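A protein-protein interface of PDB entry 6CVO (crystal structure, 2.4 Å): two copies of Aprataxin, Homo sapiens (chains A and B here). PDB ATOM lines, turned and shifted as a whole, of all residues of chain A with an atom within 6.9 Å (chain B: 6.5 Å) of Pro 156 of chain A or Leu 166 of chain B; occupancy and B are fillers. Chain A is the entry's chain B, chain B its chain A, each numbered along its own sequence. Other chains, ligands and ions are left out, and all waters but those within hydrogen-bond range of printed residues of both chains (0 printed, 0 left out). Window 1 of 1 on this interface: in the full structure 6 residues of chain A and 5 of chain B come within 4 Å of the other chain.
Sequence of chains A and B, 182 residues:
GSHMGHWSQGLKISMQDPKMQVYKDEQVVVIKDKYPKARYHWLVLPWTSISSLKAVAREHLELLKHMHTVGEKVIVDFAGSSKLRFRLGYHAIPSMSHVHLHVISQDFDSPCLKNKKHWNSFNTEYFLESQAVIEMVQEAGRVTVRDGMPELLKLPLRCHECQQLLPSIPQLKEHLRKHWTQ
ND2 of Asn 120 of chain A is in hydrogen-bond range of O of Leu 155 of chain A. NZ of Lys 116 of chain A sits at hydrogen-bond distance from O of Lys 154 of chain A, 3.0 Å away. The backbone carbonyl oxygen (O) of Leu 157 of chain B lies within hydrogen-bond range of the backbone NH (N) of Leu 166 of chain B (2.9 Å). OG of Ser 168 of chain B lies within hydrogen-bond range of N of Gln 171 of chain B, at 3.2 Å. The indole nitrogen (NE1) of Trp 119 of chain A is in hydrogen-bond range of the backbone carbonyl oxygen (O) of Arg 158 of chain A, 3.0 Å away.
Of the 16 printed residues of chain B, 5 touch a printed residue of chain A. Of the 15 printed residues of chain A, 6 touch a printed residue of chain B. Hydrophobic or aromatic side chains of chain A within 4 Å of the printed part of chain B: Leu 155, Pro 156 and Leu 165. Along chain A the printed residues that touch a printed residue of chain B span positions 116 to 165. Among the printed residues, no Asp or Glu carboxylate lies within 4 Å of a Lys or Arg side-chain nitrogen of the other chain.
Pro 156 of chain A touches Leu 166 of chain B, but with the chains exchanged Leu 166 of chain A does not touch Pro 156 of chain B (6.0 Å). Arg 158 of chain A touches Leu 165 of chain B, but with the chains exchanged Leu 165 of chain A does not touch Arg 158 of chain B (5.0 Å). Leu 165 of chain A touches Pro 156 of chain B, but with the chains exchanged Pro 156 of chain A does not touch Leu 165 of chain B (4.1 Å). 7 positions are printed for both chains.
Among the printed residues, pairs that only touch across the chains: Lys 116 of chain A with Pro 167 of chain B, Lys 154 of chain A with Pro 167 of chain B, Lys 154 of chain A with Gln 171 of chain B, Leu 155 of chain A with Leu 165 of chain B, Pro 156 of chain A with Leu 166 of chain B, Arg 158 of chain A with Leu 165 of chain B and Leu 165 of chain A with Pro 156 of chain B.
Printed residues of chain B within 4 Å of Leu 155 of chain A: Leu 165. Of chain B, only Leu 166 (3.9 Å) comes within 4 Å of Pro 156 of chain A. Leu 157 of chain A touches none of the printed residues of chain B. Cys 159 of chain A touches none of the printed residues of chain B. Of the printed residues of chain A, Pro 156 of chain B touches Leu 165 (3.8 Å). Leu 166 of chain B touches one residue of chain A. The nearest residue of chain B that does not touch Pro 156 of chain A is Leu 165 of chain B (4.1 Å). The nearest printed residue of chain A that does not touch Leu 165 of chain B is Leu 165 of chain A (4.1 Å).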
ATOM      1  N   LYS A 116      31.556 -18.320  13.313  1.00  0.00           N
ATOM      2  CA  LYS A 116      30.415 -17.428  13.141  1.00  0.00           C
ATOM      3  C   LYS A 116      30.495 -16.230  14.079  1.00  0.00           C
ATOM      4  O   LYS A 116      30.145 -15.109  13.692  1.00  0.00           O
ATOM      5  CB  LYS A 116      29.113 -18.201  13.369  1.00  0.00           C
ATOM      6  CG  LYS A 116      27.848 -17.346  13.320  1.00  0.00           C
ATOM      7  CD  LYS A 116      26.613 -18.150  13.689  1.00  0.00           C
ATOM      8  CE  LYS A 116      26.219 -19.124  12.592  1.00  0.00           C
ATOM      9  NZ  LYS A 116      25.011 -19.915  12.964  1.00  0.00           N
ATOM     10  N   TRP A 119      32.354 -13.518  12.472  1.00  0.00           N
ATOM     11  CA  TRP A 119      31.617 -12.855  11.402  1.00  0.00           C
ATOM     12  C   TRP A 119      30.558 -11.916  11.964  1.00  0.00           C
ATOM     13  O   TRP A 119      30.513 -10.730  11.614  1.00  0.00           O
ATOM     14  CB  TRP A 119      30.970 -13.891  10.483  1.00  0.00           C
ATOM     15  CG  TRP A 119      30.259 -13.256   9.336  1.00  0.00           C
ATOM     16  CD1 TRP A 119      28.911 -13.130   9.172  1.00  0.00           C
ATOM     17  CD2 TRP A 119      30.863 -12.631   8.199  1.00  0.00           C
ATOM     18  NE1 TRP A 119      28.637 -12.473   7.996  1.00  0.00           N
ATOM     19  CE2 TRP A 119      29.820 -12.156   7.380  1.00  0.00           C
ATOM     20  CE3 TRP A 119      32.185 -12.432   7.791  1.00  0.00           C
ATOM     21  CZ2 TRP A 119      30.057 -11.495   6.178  1.00  0.00           C
ATOM     22  CZ3 TRP A 119      32.419 -11.775   6.598  1.00  0.00           C
ATOM     23  CH2 TRP A 119      31.360 -11.315   5.804  1.00  0.00           C
ATOM     24  N   ASN A 120      29.692 -12.429  12.839  1.00  0.00           N
ATOM     25  CA  ASN A 120      28.563 -11.640  13.314  1.00  0.00           C
ATOM     26  C   ASN A 120      28.982 -10.529  14.268  1.00  0.00           C
ATOM     27  O   ASN A 120      28.205  -9.594  14.481  1.00  0.00           O
ATOM     28  CB  ASN A 120      27.538 -12.552  13.986  1.00  0.00           C
ATOM     29  CG  ASN A 120      26.787 -13.410  12.989  1.00  0.00           C
ATOM     30  OD1 ASN A 120      26.677 -13.060  11.814  1.00  0.00           O
ATOM     31  ND2 ASN A 120      26.265 -14.538  13.450  1.00  0.00           N
ATOM     32  N   THR A 124      26.624  -7.680  12.356  1.00  0.00           N
ATOM     33  CA  THR A 124      25.278  -7.557  12.897  1.00  0.00           C
ATOM     34  C   THR A 124      25.200  -6.277  13.717  1.00  0.00           C
ATOM     35  O   THR A 124      26.154  -5.493  13.737  1.00  0.00           O
ATOM     36  CB  THR A 124      24.910  -8.764  13.762  1.00  0.00           C
ATOM     37  OG1 THR A 124      25.687  -8.745  14.967  1.00  0.00           O
ATOM     38  CG2 THR A 124      25.161 -10.066  13.016  1.00  0.00           C
ATOM     39  N   LEU A 152      22.282 -12.491  18.508  1.00  0.00           N
ATOM     40  CA  LEU A 152      22.676 -12.068  17.168  1.00  0.00           C
ATOM     41  C   LEU A 152      23.900 -12.829  16.678  1.00  0.00           C
ATOM     42  O   LEU A 152      24.034 -13.080  15.476  1.00  0.00           O
ATOM     43  CB  LEU A 152      22.948 -10.561  17.153  1.00  0.00           C
ATOM     44  CG  LEU A 152      21.781  -9.644  17.528  1.00  0.00           C
ATOM     45  CD1 LEU A 152      22.230  -8.191  17.510  1.00  0.00           C
ATOM     46  CD2 LEU A 152      20.596  -9.849  16.598  1.00  0.00           C
ATOM     47  N   LEU A 153      24.801 -13.206  17.588  1.00  0.00           N
ATOM     48  CA  LEU A 153      26.009 -13.924  17.201  1.00  0.00           C
ATOM     49  C   LEU A 153      25.716 -15.303  16.630  1.00  0.00           C
ATOM     50  O   LEU A 153      26.605 -15.901  16.016  1.00  0.00           O
ATOM     51  CB  LEU A 153      26.945 -14.052  18.406  1.00  0.00           C
ATOM     52  CG  LEU A 153      27.434 -12.742  19.027  1.00  0.00           C
ATOM     53  CD1 LEU A 153      28.257 -13.031  20.269  1.00  0.00           C
ATOM     54  CD2 LEU A 153      28.240 -11.926  18.027  1.00  0.00           C
ATOM     55  N   LYS A 154      24.501 -15.817  16.810  1.00  0.00           N
ATOM     56  CA  LYS A 154      24.122 -17.117  16.278  1.00  0.00           C
ATOM     57  C   LYS A 154      23.412 -17.023  14.935  1.00  0.00           C
ATOM     58  O   LYS A 154      23.094 -18.060  14.346  1.00  0.00           O
ATOM     59  CB  LYS A 154      23.220 -17.846  17.277  1.00  0.00           C
ATOM     60  CG  LYS A 154      23.907 -18.234  18.574  1.00  0.00           C
ATOM     61  CD  LYS A 154      22.885 -18.597  19.637  1.00  0.00           C
ATOM     62  CE  LYS A 154      23.503 -19.407  20.761  1.00  0.00           C
ATOM     63  NZ  LYS A 154      22.479 -19.837  21.752  1.00  0.00           N
ATOM     64  N   LEU A 155      23.153 -15.817  14.444  1.00  0.00           N
ATOM     65  CA  LEU A 155      22.440 -15.667  13.184  1.00  0.00           C
ATOM     66  C   LEU A 155      23.196 -16.377  12.061  1.00  0.00           C
ATOM     67  O   LEU A 155      24.433 -16.368  12.046  1.00  0.00           O
ATOM     68  CB  LEU A 155      22.268 -14.187  12.840  1.00  0.00           C
ATOM     69  CG  LEU A 155      21.030 -13.501  13.419  1.00  0.00           C
ATOM     70  CD1 LEU A 155      21.154 -11.992  13.294  1.00  0.00           C
ATOM     71  CD2 LEU A 155      19.773 -13.991  12.718  1.00  0.00           C
ATOM     72  N   PRO A 156      22.495 -17.001  11.113  1.00  0.00           N
ATOM     73  CA  PRO A 156      23.185 -17.593   9.961  1.00  0.00           C
ATOM     74  C   PRO A 156      24.061 -16.570   9.250  1.00  0.00           C
ATOM     75  O   PRO A 156      23.789 -15.369   9.264  1.00  0.00           O
ATOM     76  CB  PRO A 156      22.035 -18.070   9.069  1.00  0.00           C
ATOM     77  CG  PRO A 156      20.923 -18.337  10.014  1.00  0.00           C
ATOM     78  CD  PRO A 156      21.056 -17.320  11.112  1.00  0.00           C
ATOM     79  N   LEU A 157      25.126 -17.065   8.625  1.00  0.00           N
ATOM     80  CA  LEU A 157      26.067 -16.195   7.935  1.00  0.00           C
ATOM     81  C   LEU A 157      25.385 -15.495   6.767  1.00  0.00           C
ATOM     82  O   LEU A 157      24.696 -16.127   5.962  1.00  0.00           O
ATOM     83  CB  LEU A 157      27.260 -17.010   7.440  1.00  0.00           C
ATOM     84  CG  LEU A 157      27.999 -17.812   8.511  1.00  0.00           C
ATOM     85  CD1 LEU A 157      28.901 -18.853   7.871  1.00  0.00           C
ATOM     86  CD2 LEU A 157      28.804 -16.888   9.414  1.00  0.00           C
ATOM     87  N   ARG A 158      25.581 -14.180   6.677  1.00  0.00           N
ATOM     88  CA  ARG A 158      25.018 -13.372   5.602  1.00  0.00           C
ATOM     89  C   ARG A 158      26.119 -12.506   5.014  1.00  0.00           C
ATOM     90  O   ARG A 158      26.786 -11.766   5.745  1.00  0.00           O
ATOM     91  CB  ARG A 158      23.867 -12.495   6.106  1.00  0.00           C
ATOM     92  CG  ARG A 158      23.221 -11.644   5.020  1.00  0.00           C
ATOM     93  CD  ARG A 158      22.230 -10.643   5.591  1.00  0.00           C
ATOM     94  NE  ARG A 158      21.085 -11.295   6.221  1.00  0.00           N
ATOM     95  CZ  ARG A 158      20.058 -11.817   5.556  1.00  0.00           C
ATOM     96  NH1 ARG A 158      19.060 -12.388   6.217  1.00  0.00           N
ATOM     97  NH2 ARG A 158      20.027 -11.780   4.231  1.00  0.00           N
ATOM     98  N   CYS A 159      26.306 -12.596   3.700  1.00  0.00           N
ATOM     99  CA  CYS A 159      27.267 -11.740   3.021  1.00  0.00           C
ATOM    100  C   CYS A 159      26.884 -10.278   3.196  1.00  0.00           C
ATOM    101  O   CYS A 159      25.734  -9.892   2.969  1.00  0.00           O
ATOM    102  CB  CYS A 159      27.333 -12.096   1.537  1.00  0.00           C
ATOM    103  SG  CYS A 159      28.419 -11.022   0.571  1.00  0.00           S
ATOM    104  N   LEU A 165      22.758 -15.592   2.070  1.00  0.00           N
ATOM    105  CA  LEU A 165      22.958 -16.410   3.258  1.00  0.00           C
ATOM    106  C   LEU A 165      23.813 -17.621   2.909  1.00  0.00           C
ATOM    107  O   LEU A 165      23.558 -18.301   1.909  1.00  0.00           O
ATOM    108  CB  LEU A 165      21.611 -16.857   3.830  1.00  0.00           C
ATOM    109  CG  LEU A 165      20.718 -15.719   4.326  1.00  0.00           C
ATOM    110  CD1 LEU A 165      19.275 -16.171   4.454  1.00  0.00           C
ATOM    111  CD2 LEU A 165      21.231 -15.192   5.652  1.00  0.00           C
ATOM    112  N   LEU A 166      24.832 -17.881   3.728  1.00  0.00           N
ATOM    113  CA  LEU A 166      25.746 -18.986   3.493  1.00  0.00           C
ATOM    114  C   LEU A 166      25.686 -19.983   4.646  1.00  0.00           C
ATOM    115  O   LEU A 166      25.533 -19.579   5.803  1.00  0.00           O
ATOM    116  CB  LEU A 166      27.192 -18.484   3.324  1.00  0.00           C
ATOM    117  CG  LEU A 166      27.577 -17.846   1.982  1.00  0.00           C
ATOM    118  CD1 LEU A 166      27.288 -18.780   0.810  1.00  0.00           C
ATOM    119  CD2 LEU A 166      26.898 -16.497   1.774  1.00  0.00           C
ATOM    120  N   PRO A 167      25.814 -21.285   4.367  1.00  0.00           N
ATOM    121  CA  PRO A 167      25.622 -22.288   5.423  1.00  0.00           C
ATOM    122  C   PRO A 167      26.847 -22.555   6.284  1.00  0.00           C
ATOM    123  O   PRO A 167      26.701 -23.164   7.353  1.00  0.00           O
ATOM    124  CB  PRO A 167      25.235 -23.542   4.631  1.00  0.00           C
ATOM    125  CG  PRO A 167      25.974 -23.394   3.345  1.00  0.00           C
ATOM    126  CD  PRO A 167      26.043 -21.913   3.052  1.00  0.00           C
ATOM    127  N   PRO B 156      17.685 -21.607   4.552  1.00  0.00           N
ATOM    128  CA  PRO B 156      17.925 -21.484   5.994  1.00  0.00           C
ATOM    129  C   PRO B 156      16.619 -21.496   6.777  1.00  0.00           C
ATOM    130  O   PRO B 156      15.573 -21.057   6.292  1.00  0.00           O
ATOM    131  CB  PRO B 156      18.647 -20.139   6.117  1.00  0.00           C
ATOM    132  CG  PRO B 156      19.332 -19.972   4.807  1.00  0.00           C
ATOM    133  CD  PRO B 156      18.417 -20.583   3.785  1.00  0.00           C
ATOM    134  N   LEU B 157      16.691 -22.008   8.002  1.00  0.00           N
ATOM    135  CA  LEU B 157      15.501 -22.138   8.833  1.00  0.00           C
ATOM    136  C   LEU B 157      14.964 -20.763   9.212  1.00  0.00           C
ATOM    137  O   LEU B 157      15.710 -19.903   9.692  1.00  0.00           O
ATOM    138  CB  LEU B 157      15.826 -22.944  10.091  1.00  0.00           C
ATOM    139  CG  LEU B 157      16.366 -24.357   9.853  1.00  0.00           C
ATOM    140  CD1 LEU B 157      16.880 -24.948  11.153  1.00  0.00           C
ATOM    141  CD2 LEU B 157      15.298 -25.252   9.245  1.00  0.00           C
ATOM    142  N   ARG B 158      13.665 -20.560   8.996  1.00  0.00           N
ATOM    143  CA  ARG B 158      13.001 -19.311   9.335  1.00  0.00           C
ATOM    144  C   ARG B 158      11.712 -19.629  10.076  1.00  0.00           C
ATOM    145  O   ARG B 158      10.958 -20.517   9.665  1.00  0.00           O
ATOM    146  CB  ARG B 158      12.700 -18.479   8.084  1.00  0.00           C
ATOM    147  CG  ARG B 158      12.172 -17.085   8.391  1.00  0.00           C
ATOM    148  CD  ARG B 158      11.755 -16.342   7.129  1.00  0.00           C
ATOM    149  NE  ARG B 158      12.896 -15.970   6.294  1.00  0.00           N
ATOM    150  CZ  ARG B 158      13.680 -14.917   6.517  1.00  0.00           C
ATOM    151  NH1 ARG B 158      13.462 -14.126   7.558  1.00  0.00           N
ATOM    152  NH2 ARG B 158      14.691 -14.657   5.698  1.00  0.00           N
ATOM    153  N   CYS B 159      11.469 -18.913  11.169  1.00  0.00           N
ATOM    154  CA  CYS B 159      10.255 -19.120  11.943  1.00  0.00           C
ATOM    155  C   CYS B 159       9.036 -18.649  11.162  1.00  0.00           C
ATOM    156  O   CYS B 159       9.033 -17.569  10.568  1.00  0.00           O
ATOM    157  CB  CYS B 159      10.337 -18.379  13.274  1.00  0.00           C
ATOM    158  SG  CYS B 159       8.862 -18.570  14.300  1.00  0.00           S
ATOM    159  N   CYS B 162       7.216 -15.433  13.449  1.00  0.00           N
ATOM    160  CA  CYS B 162       7.860 -14.130  13.532  1.00  0.00           C
ATOM    161  C   CYS B 162       8.893 -13.893  12.440  1.00  0.00           C
ATOM    162  O   CYS B 162       9.441 -12.787  12.361  1.00  0.00           O
ATOM    163  CB  CYS B 162       8.525 -13.955  14.905  1.00  0.00           C
ATOM    164  SG  CYS B 162      10.014 -14.942  15.140  1.00  0.00           S
ATOM    165  N   GLN B 163       9.179 -14.888  11.600  1.00  0.00           N
ATOM    166  CA  GLN B 163      10.081 -14.771  10.450  1.00  0.00           C
ATOM    167  C   GLN B 163      11.551 -14.725  10.849  1.00  0.00           C
ATOM    168  O   GLN B 163      12.400 -14.444   9.989  1.00  0.00           O
ATOM    169  CB  GLN B 163       9.774 -13.533   9.602  1.00  0.00           C
ATOM    170  CG  GLN B 163       8.312 -13.396   9.211  1.00  0.00           C
ATOM    171  CD  GLN B 163       7.802 -14.598   8.444  1.00  0.00           C
ATOM    172  OE1 GLN B 163       8.555 -15.256   7.726  1.00  0.00           O
ATOM    173  NE2 GLN B 163       6.518 -14.897   8.599  1.00  0.00           N
ATOM    174  N   GLN B 164      11.888 -14.992  12.108  1.00  0.00           N
ATOM    175  CA  GLN B 164      13.281 -14.937  12.531  1.00  0.00           C
ATOM    176  C   GLN B 164      14.063 -16.118  11.966  1.00  0.00           C
ATOM    177  O   GLN B 164      13.566 -17.246  11.918  1.00  0.00           O
ATOM    178  CB  GLN B 164      13.371 -14.930  14.057  1.00  0.00           C
ATOM    179  CG  GLN B 164      14.790 -14.829  14.595  1.00  0.00           C
ATOM    180  CD  GLN B 164      14.832 -14.630  16.098  1.00  0.00           C
ATOM    181  OE1 GLN B 164      13.926 -14.036  16.682  1.00  0.00           O
ATOM    182  NE2 GLN B 164      15.887 -15.131  16.732  1.00  0.00           N
ATOM    183  N   LEU B 165      15.293 -15.848  11.534  1.00  0.00           N
ATOM    184  CA  LEU B 165      16.175 -16.894  11.035  1.00  0.00           C
ATOM    185  C   LEU B 165      16.845 -17.609  12.202  1.00  0.00           C
ATOM    186  O   LEU B 165      17.373 -16.966  13.114  1.00  0.00           O
ATOM    187  CB  LEU B 165      17.238 -16.301  10.108  1.00  0.00           C
ATOM    188  CG  LEU B 165      16.774 -15.745   8.760  1.00  0.00           C
ATOM    189  CD1 LEU B 165      17.907 -14.979   8.094  1.00  0.00           C
ATOM    190  CD2 LEU B 165      16.282 -16.860   7.853  1.00  0.00           C
ATOM    191  N   LEU B 166      16.821 -18.940  12.172  1.00  0.00           N
ATOM    192  CA  LEU B 166      17.490 -19.742  13.183  1.00  0.00           C
ATOM    193  C   LEU B 166      18.570 -20.602  12.536  1.00  0.00           C
ATOM    194  O   LEU B 166      18.430 -21.014  11.380  1.00  0.00           O
ATOM    195  CB  LEU B 166      16.503 -20.645  13.936  1.00  0.00           C
ATOM    196  CG  LEU B 166      15.481 -19.979  14.866  1.00  0.00           C
ATOM    197  CD1 LEU B 166      16.133 -18.955  15.791  1.00  0.00           C
ATOM    198  CD2 LEU B 166      14.340 -19.347  14.082  1.00  0.00           C
ATOM    199  N   PRO B 167      19.660 -20.892  13.254  1.00  0.00           N
ATOM    200  CA  PRO B 167      20.792 -21.595  12.640  1.00  0.00           C
ATOM    201  C   PRO B 167      20.711 -23.113  12.643  1.00  0.00           C
ATOM    202  O   PRO B 167      21.505 -23.746  11.932  1.00  0.00           O
ATOM    203  CB  PRO B 167      21.970 -21.124  13.502  1.00  0.00           C
ATOM    204  CG  PRO B 167      21.375 -20.960  14.853  1.00  0.00           C
ATOM    205  CD  PRO B 167      19.957 -20.486  14.641  1.00  0.00           C
ATOM    206  N   SER B 168      19.803 -23.717  13.405  1.00  0.00           N
ATOM    207  CA  SER B 168      19.768 -25.170  13.509  1.00  0.00           C
ATOM    208  C   SER B 168      18.367 -25.618  13.897  1.00  0.00           C
ATOM    209  O   SER B 168      17.549 -24.828  14.378  1.00  0.00           O
ATOM    210  CB  SER B 168      20.790 -25.680  14.530  1.00  0.00           C
ATOM    211  OG  SER B 168      20.401 -25.344  15.850  1.00  0.00           O
ATOM    212  N   ILE B 169      18.107 -26.908  13.678  1.00  0.00           N
ATOM    213  CA  ILE B 169      16.826 -27.490  14.084  1.00  0.00           C
ATOM    214  C   ILE B 169      16.644 -27.421  15.595  1.00  0.00           C
ATOM    215  O   ILE B 169      15.577 -26.974  16.049  1.00  0.00           O
ATOM    216  CB  ILE B 169      16.696 -28.917  13.535  1.00  0.00           C
ATOM    217  CG1 ILE B 169      16.493 -28.898  12.013  1.00  0.00           C
ATOM    218  CG2 ILE B 169      15.564 -29.689  14.230  1.00  0.00           C
ATOM    219  CD1 ILE B 169      15.135 -28.380  11.554  1.00  0.00           C
ATOM    220  N   GLN B 171      17.840 -25.309  17.826  1.00  0.00           N
ATOM    221  CA  GLN B 171      17.572 -23.930  18.222  1.00  0.00           C
ATOM    222  C   GLN B 171      16.229 -23.448  17.690  1.00  0.00           C
ATOM    223  O   GLN B 171      15.592 -22.589  18.310  1.00  0.00           O
ATOM    224  CB  GLN B 171      18.697 -23.014  17.741  1.00  0.00           C
ATOM    225  CG  GLN B 171      19.938 -23.068  18.616  1.00  0.00           C
ATOM    226  CD  GLN B 171      21.091 -22.263  18.050  1.00  0.00           C
ATOM    227  OE1 GLN B 171      20.983 -21.051  17.859  1.00  0.00           O
ATOM    228  NE2 GLN B 171      22.202 -22.936  17.777  1.00  0.00           N
ATOM    229  N   LEU B 172      15.784 -23.979  16.550  1.00  0.00           N
ATOM    230  CA  LEU B 172      14.444 -23.663  16.067  1.00  0.00           C
ATOM    231  C   LEU B 172      13.382 -24.222  17.005  1.00  0.00           C
ATOM    232  O   LEU B 172      12.433 -23.521  17.374  1.00  0.00           O
ATOM    233  CB  LEU B 172      14.251 -24.207  14.651  1.00  0.00           C
ATOM    234  CG  LEU B 172      12.817 -24.167  14.110  1.00  0.00           C
ATOM    235  CD1 LEU B 172      12.242 -22.759  14.181  1.00  0.00           C
ATOM    236  CD2 LEU B 172      12.768 -24.691  12.687  1.00  0.00           C
ATOM    237  N   LYS B 173      13.529 -25.487  17.404  1.00  0.00           N
ATOM    238  CA  LYS B 173      12.550 -26.099  18.295  1.00  0.00           C
ATOM    239  C   LYS B 173      12.480 -25.360  19.626  1.00  0.00           C
ATOM    240  O   LYS B 173      11.400 -25.229  20.215  1.00  0.00           O
ATOM    241  CB  LYS B 173      12.890 -27.573  18.514  1.00  0.00           C
ATOM    242  CG  LYS B 173      12.748 -28.423  17.263  1.00  0.00           C
ATOM    243  CD  LYS B 173      12.765 -29.904  17.595  1.00  0.00           C
ATOM    244  CE  LYS B 173      12.441 -30.750  16.376  1.00  0.00           C
ATOM    245  NZ  LYS B 173      12.035 -32.130  16.752  1.00  0.00           N
ATOM    246  N   HIS B 175      13.168 -22.123  19.913  1.00  0.00           N
ATOM    247  CA  HIS B 175      12.518 -20.862  19.577  1.00  0.00           C
ATOM    248  C   HIS B 175      11.004 -21.020  19.508  1.00  0.00           C
ATOM    249  O   HIS B 175      10.259 -20.152  19.977  1.00  0.00           O
ATOM    250  CB  HIS B 175      13.062 -20.336  18.250  1.00  0.00           C
ATOM    251  CG  HIS B 175      12.339 -19.132  17.735  1.00  0.00           C
ATOM    252  ND1 HIS B 175      12.710 -17.845  18.060  1.00  0.00           N
ATOM    253  CD2 HIS B 175      11.264 -19.019  16.920  1.00  0.00           C
ATOM    254  CE1 HIS B 175      11.896 -16.991  17.465  1.00  0.00           C
ATOM    255  NE2 HIS B 175      11.010 -17.678  16.768  1.00  0.00           N
